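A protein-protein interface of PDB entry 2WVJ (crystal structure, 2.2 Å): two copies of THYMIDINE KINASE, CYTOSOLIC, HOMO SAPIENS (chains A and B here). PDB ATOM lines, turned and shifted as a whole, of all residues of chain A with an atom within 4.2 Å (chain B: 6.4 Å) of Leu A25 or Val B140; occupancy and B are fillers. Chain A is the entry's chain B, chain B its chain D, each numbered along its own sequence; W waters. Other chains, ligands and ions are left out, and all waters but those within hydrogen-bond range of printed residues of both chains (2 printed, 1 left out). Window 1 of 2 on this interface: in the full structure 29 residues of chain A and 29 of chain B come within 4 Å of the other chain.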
ATOM      1  N   VAL A  23      12.690  -9.684  15.659  1.00  0.00           N
ATOM      2  CA  VAL A  23      13.457 -10.753  16.284  1.00  0.00           C
ATOM      3  C   VAL A  23      12.724 -12.093  16.160  1.00  0.00           C
ATOM      4  O   VAL A  23      11.573 -12.230  16.588  1.00  0.00           O
ATOM      5  CB  VAL A  23      13.767 -10.430  17.777  1.00  0.00           C
ATOM      6  CG1 VAL A  23      14.551 -11.557  18.426  1.00  0.00           C
ATOM      7  CG2 VAL A  23      14.537  -9.106  17.911  1.00  0.00           C
ATOM      8  N   ILE A  24      13.401 -13.068  15.555  1.00  0.00           N
ATOM      9  CA  ILE A  24      12.893 -14.432  15.432  1.00  0.00           C
ATOM     10  C   ILE A  24      13.675 -15.330  16.398  1.00  0.00           C
ATOM     11  O   ILE A  24      14.842 -15.663  16.165  1.00  0.00           O
ATOM     12  CB  ILE A  24      13.022 -14.967  13.974  1.00  0.00           C
ATOM     13  CG1 ILE A  24      12.488 -13.945  12.956  1.00  0.00           C
ATOM     14  CG2 ILE A  24      12.343 -16.335  13.826  1.00  0.00           C
ATOM     15  CD1 ILE A  24      13.068 -14.106  11.557  1.00  0.00           C
ATOM     16  N   LEU A  25      13.029 -15.697  17.496  1.00  0.00           N
ATOM     17  CA  LEU A  25      13.655 -16.546  18.502  1.00  0.00           C
ATOM     18  C   LEU A  25      13.156 -17.979  18.354  1.00  0.00           C
ATOM     19  O   LEU A  25      12.215 -18.244  17.605  1.00  0.00           O
ATOM     20  CB  LEU A  25      13.365 -16.020  19.918  1.00  0.00           C
ATOM     21  CG  LEU A  25      13.868 -14.620  20.321  1.00  0.00           C
ATOM     22  CD1 LEU A  25      13.271 -14.180  21.654  1.00  0.00           C
ATOM     23  CD2 LEU A  25      15.401 -14.531  20.361  1.00  0.00           C
ATOM     24  N   GLY A  26      13.797 -18.893  19.074  1.00  0.00           N
ATOM     25  CA  GLY A  26      13.369 -20.276  19.123  1.00  0.00           C
ATOM     26  C   GLY A  26      14.512 -21.219  19.448  1.00  0.00           C
ATOM     27  O   GLY A  26      15.672 -20.803  19.480  1.00  0.00           O
ATOM     28  N   LYS A  32      14.399 -21.049  12.162  1.00  0.00           N
ATOM     29  CA  LYS A  32      14.617 -19.601  12.309  1.00  0.00           C
ATOM     30  C   LYS A  32      15.263 -18.947  11.066  1.00  0.00           C
ATOM     31  O   LYS A  32      14.874 -17.838  10.687  1.00  0.00           O
ATOM     32  CB  LYS A  32      15.454 -19.296  13.558  1.00  0.00           C
ATOM     33  CG  LYS A  32      14.871 -19.825  14.877  1.00  0.00           C
ATOM     34  CD  LYS A  32      15.764 -19.512  16.079  1.00  0.00           C
ATOM     35  CE  LYS A  32      17.187 -20.080  15.944  1.00  0.00           C
ATOM     36  NZ  LYS A  32      17.207 -21.566  15.941  1.00  0.00           N
ATOM     37  N   ALA A 123      17.846 -15.932  15.829  1.00  0.00           N
ATOM     38  CA  ALA A 123      18.711 -16.258  16.963  1.00  0.00           C
ATOM     39  C   ALA A 123      18.091 -17.258  17.934  1.00  0.00           C
ATOM     40  O   ALA A 123      16.872 -17.280  18.136  1.00  0.00           O
ATOM     41  CB  ALA A 123      19.103 -14.982  17.713  1.00  0.00           C
ATOM     42  N   ASP A 125      17.230 -18.171  21.616  1.00  0.00           N
ATOM     43  CA  ASP A 125      16.984 -17.395  22.828  1.00  0.00           C
ATOM     44  C   ASP A 125      17.778 -17.962  24.012  1.00  0.00           C
ATOM     45  O   ASP A 125      18.256 -17.214  24.876  1.00  0.00           O
ATOM     46  CB  ASP A 125      15.485 -17.292  23.148  1.00  0.00           C
ATOM     47  CG  ASP A 125      14.802 -18.648  23.282  1.00  0.00           C
ATOM     48  OD1 ASP A 125      13.996 -18.803  24.229  1.00  0.00           O
ATOM     49  OD2 ASP A 125      15.049 -19.554  22.450  1.00  0.00           O
ATOM     50  N   LEU A 137      18.740 -11.272  24.264  1.00  0.00           N
ATOM     51  CA  LEU A 137      17.449 -10.866  24.813  1.00  0.00           C
ATOM     52  C   LEU A 137      17.372  -9.365  25.090  1.00  0.00           C
ATOM     53  O   LEU A 137      16.281  -8.815  25.212  1.00  0.00           O
ATOM     54  CB  LEU A 137      17.068 -11.705  26.038  1.00  0.00           C
ATOM     55  CG  LEU A 137      16.892 -13.215  25.787  1.00  0.00           C
ATOM     56  CD1 LEU A 137      16.465 -13.929  27.065  1.00  0.00           C
ATOM     57  CD2 LEU A 137      15.911 -13.524  24.645  1.00  0.00           C
ATOM     58  N   VAL A 146       8.635  -9.346  18.044  1.00  0.00           N
ATOM     59  CA  VAL A 146       9.338 -10.483  18.646  1.00  0.00           C
ATOM     60  C   VAL A 146       8.471 -11.738  18.607  1.00  0.00           C
ATOM     61  O   VAL A 146       7.329 -11.732  19.079  1.00  0.00           O
ATOM     62  CB  VAL A 146       9.773 -10.209  20.116  1.00  0.00           C
ATOM     63  CG1 VAL A 146      10.459 -11.441  20.723  1.00  0.00           C
ATOM     64  CG2 VAL A 146      10.689  -8.984  20.209  1.00  0.00           C
ATOM     65  N   VAL A 147       9.032 -12.815  18.062  1.00  0.00           N
ATOM     66  CA  VAL A 147       8.355 -14.103  18.031  1.00  0.00           C
ATOM     67  C   VAL A 147       9.274 -15.223  18.557  1.00  0.00           C
ATOM     68  O   VAL A 147      10.500 -15.157  18.409  1.00  0.00           O
ATOM     69  CB  VAL A 147       7.826 -14.414  16.592  1.00  0.00           C
ATOM     70  CG1 VAL A 147       8.902 -15.034  15.707  1.00  0.00           C
ATOM     71  CG2 VAL A 147       6.646 -15.318  16.652  1.00  0.00           C
ATOM     72  N   LYS A 148       8.680 -16.231  19.192  1.00  0.00           N
ATOM     73  CA  LYS A 148       9.406 -17.450  19.496  1.00  0.00           C
ATOM     74  C   LYS A 148       8.794 -18.634  18.751  1.00  0.00           C
ATOM     75  O   LYS A 148       7.626 -18.980  18.958  1.00  0.00           O
ATOM     76  CB  LYS A 148       9.496 -17.728  21.004  1.00  0.00           C
ATOM     77  CG  LYS A 148      10.341 -18.965  21.294  1.00  0.00           C
ATOM     78  CD  LYS A 148      10.748 -19.135  22.747  1.00  0.00           C
ATOM     79  CE  LYS A 148      11.530 -20.448  22.886  1.00  0.00           C
ATOM     80  NZ  LYS A 148      11.801 -20.831  24.296  1.00  0.00           N
ATOM     81  N   LEU A 149       9.599 -19.237  17.883  1.00  0.00           N
ATOM     82  CA  LEU A 149       9.176 -20.383  17.087  1.00  0.00           C
ATOM     83  C   LEU A 149       9.273 -21.675  17.881  1.00  0.00           C
ATOM     84  O   LEU A 149       9.919 -21.727  18.926  1.00  0.00           O
ATOM     85  CB  LEU A 149      10.010 -20.503  15.804  1.00  0.00           C
ATOM     86  CG  LEU A 149      10.007 -19.349  14.795  1.00  0.00           C
ATOM     87  CD1 LEU A 149      10.808 -19.751  13.562  1.00  0.00           C
ATOM     88  CD2 LEU A 149       8.599 -18.896  14.414  1.00  0.00           C
ATOM     89  N   VAL B  23       4.377 -16.443  27.842  1.00  0.00           N
ATOM     90  CA  VAL B  23       4.718 -15.060  28.155  1.00  0.00           C
ATOM     91  C   VAL B  23       4.071 -14.106  27.153  1.00  0.00           C
ATOM     92  O   VAL B  23       4.200 -14.286  25.935  1.00  0.00           O
ATOM     93  CB  VAL B  23       6.258 -14.814  28.234  1.00  0.00           C
ATOM     94  CG1 VAL B  23       6.547 -13.409  28.748  1.00  0.00           C
ATOM     95  CG2 VAL B  23       6.939 -15.830  29.150  1.00  0.00           C
ATOM     96  N   LEU B  25       4.349 -10.336  26.252  1.00  0.00           N
ATOM     97  CA  LEU B  25       5.095  -9.088  26.332  1.00  0.00           C
ATOM     98  C   LEU B  25       4.431  -7.972  25.524  1.00  0.00           C
ATOM     99  O   LEU B  25       3.470  -8.201  24.800  1.00  0.00           O
ATOM    100  CB  LEU B  25       6.547  -9.286  25.873  1.00  0.00           C
ATOM    101  CG  LEU B  25       7.408 -10.285  26.661  1.00  0.00           C
ATOM    102  CD1 LEU B  25       8.734 -10.526  25.947  1.00  0.00           C
ATOM    103  CD2 LEU B  25       7.637  -9.829  28.110  1.00  0.00           C
ATOM    104  N   ILE B 136      12.330 -10.120  33.976  1.00  0.00           N
ATOM    105  CA  ILE B 136      11.301 -10.677  33.085  1.00  0.00           C
ATOM    106  C   ILE B 136      11.817 -11.471  31.873  1.00  0.00           C
ATOM    107  O   ILE B 136      11.245 -12.504  31.521  1.00  0.00           O
ATOM    108  CB  ILE B 136      10.252  -9.604  32.644  1.00  0.00           C
ATOM    109  CG1 ILE B 136       8.987 -10.280  32.110  1.00  0.00           C
ATOM    110  CG2 ILE B 136      10.840  -8.627  31.617  1.00  0.00           C
ATOM    111  CD1 ILE B 136       8.302 -11.202  33.106  1.00  0.00           C
ATOM    112  N   LEU B 137      12.900 -11.005  31.253  1.00  0.00           N
ATOM    113  CA  LEU B 137      13.404 -11.650  30.037  1.00  0.00           C
ATOM    114  C   LEU B 137      14.067 -13.008  30.295  1.00  0.00           C
ATOM    115  O   LEU B 137      14.201 -13.818  29.379  1.00  0.00           O
ATOM    116  CB  LEU B 137      14.330 -10.715  29.245  1.00  0.00           C
ATOM    117  CG  LEU B 137      13.727  -9.409  28.704  1.00  0.00           C
ATOM    118  CD1 LEU B 137      14.774  -8.604  27.952  1.00  0.00           C
ATOM    119  CD2 LEU B 137      12.512  -9.638  27.828  1.00  0.00           C
ATOM    120  N   ASN B 138      14.458 -13.261  31.542  1.00  0.00           N
ATOM    121  CA  ASN B 138      14.980 -14.570  31.934  1.00  0.00           C
ATOM    122  C   ASN B 138      13.949 -15.694  31.788  1.00  0.00           C
ATOM    123  O   ASN B 138      14.312 -16.872  31.732  1.00  0.00           O
ATOM    124  CB  ASN B 138      15.540 -14.535  33.361  1.00  0.00           C
ATOM    125  CG  ASN B 138      16.810 -13.704  33.472  1.00  0.00           C
ATOM    126  OD1 ASN B 138      17.603 -13.635  32.535  1.00  0.00           O
ATOM    127  ND2 ASN B 138      17.008 -13.072  34.626  1.00  0.00           N
ATOM    128  N   LEU B 139      12.670 -15.320  31.722  1.00  0.00           N
ATOM    129  CA  LEU B 139      11.596 -16.269  31.424  1.00  0.00           C
ATOM    130  C   LEU B 139      11.634 -16.806  29.997  1.00  0.00           C
ATOM    131  O   LEU B 139      11.176 -17.918  29.746  1.00  0.00           O
ATOM    132  CB  LEU B 139      10.217 -15.645  31.674  1.00  0.00           C
ATOM    133  CG  LEU B 139       9.686 -15.588  33.106  1.00  0.00           C
ATOM    134  CD1 LEU B 139       8.277 -15.045  33.079  1.00  0.00           C
ATOM    135  CD2 LEU B 139       9.716 -16.954  33.771  1.00  0.00           C
ATOM    136  N   VAL B 140      12.160 -16.010  29.070  1.00  0.00           N
ATOM    137  CA  VAL B 140      12.058 -16.311  27.636  1.00  0.00           C
ATOM    138  C   VAL B 140      12.681 -17.667  27.233  1.00  0.00           C
ATOM    139  O   VAL B 140      11.997 -18.468  26.577  1.00  0.00           O
ATOM    140  CB  VAL B 140      12.519 -15.109  26.746  1.00  0.00           C
ATOM    141  CG1 VAL B 140      12.554 -15.486  25.277  1.00  0.00           C
ATOM    142  CG2 VAL B 140      11.585 -13.921  26.951  1.00  0.00           C
ATOM    143  N   PRO B 141      13.947 -17.944  27.645  1.00  0.00           N
ATOM    144  CA  PRO B 141      14.540 -19.268  27.403  1.00  0.00           C
ATOM    145  C   PRO B 141      13.824 -20.406  28.147  1.00  0.00           C
ATOM    146  O   PRO B 141      13.987 -21.575  27.792  1.00  0.00           O
ATOM    147  CB  PRO B 141      15.968 -19.117  27.945  1.00  0.00           C
ATOM    148  CG  PRO B 141      16.229 -17.657  27.960  1.00  0.00           C
ATOM    149  CD  PRO B 141      14.906 -17.059  28.332  1.00  0.00           C
ATOM    150  N   LEU B 142      13.041 -20.057  29.167  1.00  0.00           N
ATOM    151  CA  LEU B 142      12.293 -21.042  29.947  1.00  0.00           C
ATOM    152  C   LEU B 142      10.881 -21.315  29.404  1.00  0.00           C
ATOM    153  O   LEU B 142      10.220 -22.257  29.833  1.00  0.00           O
ATOM    154  CB  LEU B 142      12.199 -20.594  31.409  1.00  0.00           C
ATOM    155  CG  LEU B 142      13.484 -20.315  32.193  1.00  0.00           C
ATOM    156  CD1 LEU B 142      13.124 -19.789  33.558  1.00  0.00           C
ATOM    157  CD2 LEU B 142      14.352 -21.570  32.312  1.00  0.00           C
ATOM    158  N   ALA B 143      10.433 -20.494  28.457  1.00  0.00           N
ATOM    159  CA  ALA B 143       9.026 -20.476  28.049  1.00  0.00           C
ATOM    160  C   ALA B 143       8.757 -21.199  26.732  1.00  0.00           C
ATOM    161  O   ALA B 143       9.523 -21.084  25.777  1.00  0.00           O
ATOM    162  CB  ALA B 143       8.531 -19.043  27.969  1.00  0.00           C
ATOM    163  N   GLU B 144       7.657 -21.943  26.681  1.00  0.00           N
ATOM    164  CA  GLU B 144       7.287 -22.601  25.439  1.00  0.00           C
ATOM    165  C   GLU B 144       6.560 -21.667  24.470  1.00  0.00           C
ATOM    166  O   GLU B 144       6.611 -21.866  23.256  1.00  0.00           O
ATOM    167  CB  GLU B 144       6.559 -23.937  25.662  1.00  0.00           C
ATOM    168  CG  GLU B 144       5.821 -24.091  26.971  1.00  0.00           C
ATOM    169  CD  GLU B 144       6.706 -24.520  28.135  1.00  0.00           C
ATOM    170  OE1 GLU B 144       6.958 -25.735  28.300  1.00  0.00           O
ATOM    171  OE2 GLU B 144       7.115 -23.632  28.908  1.00  0.00           O
ATOM    172  N   VAL B 146       6.182 -17.382  23.599  1.00  0.00           N
ATOM    173  CA  VAL B 146       6.518 -15.966  23.803  1.00  0.00           C
ATOM    174  C   VAL B 146       5.985 -15.110  22.653  1.00  0.00           C
ATOM    175  O   VAL B 146       6.206 -15.416  21.479  1.00  0.00           O
ATOM    176  CB  VAL B 146       8.052 -15.719  23.986  1.00  0.00           C
ATOM    177  CG1 VAL B 146       8.335 -14.236  24.200  1.00  0.00           C
ATOM    178  CG2 VAL B 146       8.623 -16.529  25.160  1.00  0.00           C
HETATM  179  O   HOH W   1       5.926 -18.601  20.926  1.00  0.00           O
HETATM  180  O   HOH W   2       8.749 -22.805  21.449  1.00  0.00           O
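NZ of Lys A148 is in salt-bridge range of OD1 of Asp A125.
N of Leu A149 lies within hydrogen-bond range of O of Leu A25 (2.8 Å).
O of Val A147 sits at hydrogen-bond distance from N of Leu A25, 2.7 Å away.
Of chain B, only Val B140 comes within 4 Å of Leu A25.
Val B140 touches just these residues of chain A: Leu A25 (3.9 Å), Asp A125 (3.1 Å), Leu A137 (3.9 Å) and Lys A148 (3.3 Å).
Printed residues of chain A within 4 Å of Pro B141: Asp A125 (3.3 Å) and Leu A137 (3.7 Å).
Printed residues of chain B within 4 Å of Leu A137: Leu B137, Val B140 and Pro B141.
Printed residues of chain A within 4 Å of Leu B137: Leu A137 (3.1 Å).
Printed residues of chain B within 4 Å of Asp A125: Val B140 (3.1 Å) and Pro B141 (3.3 Å).
Of the printed residues of chain A, Ala B143 touches Lys A148 (2.7 Å).
Leu B139 touches none of the printed residues of chain A.
The nearest printed residue of chain A that does not touch Val B140 is Val A146 (6.4 Å).
Of the 12 printed residues of chain A, 4 touch a printed residue of chain B.
Hydrophobic or aromatic side chains of chain A within 4 Å of the printed part of chain B: Leu A25 and Leu A137.
Printed residues of chain B that touch a printed residue of chain A: Leu B137, Val B140, Pro B141, Ala B143 and Val B146.
Along chain B the printed residues that touch a printed residue of chain A span positions 137 to 146.
Among the printed residues, 9 pairs touch across the chains.
The side-chain amino group (NZ) of Lys A148 sits at hydrogen-bond distance from the backbone carbonyl oxygen (O) of Val B140 (3.3 Å).
The side-chain amino group (NZ) of Lys A148 lies within hydrogen-bond range of the backbone carbonyl oxygen (O) of Ala B143 (2.7 Å).
O of Val B140 lies close to OD1 of Asp A125, at 3.1 Å.
The backbone NH (N) of Lys A148 sits at hydrogen-bond distance from the backbone carbonyl oxygen (O) of Val B146, 3.5 Å away.
Leu A137 touches its own counterpart, Leu B137.
Positions printed for both chains: 23, 25, 137 and 146.
Among the printed residues, pairs that only touch across the chains: Leu A137 with Leu B137 (3.1 Å), Asp A125 with Pro B141 (3.3 Å), Leu A137 with Pro B141 (3.7 Å), Leu A25 with Val B140 (3.9 Å) and Leu A137 with Val B140 (3.9 Å).
Water W1 lies within hydrogen-bond range of the backbone carbonyl oxygen of Lys A148 (2.6 Å) and the backbone NH of Val B146 (2.9 Å).
Water W2 bridges the backbone carbonyl oxygen (O) of Glu B144 and the backbone carbonyl oxygen (O) of Leu A149.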
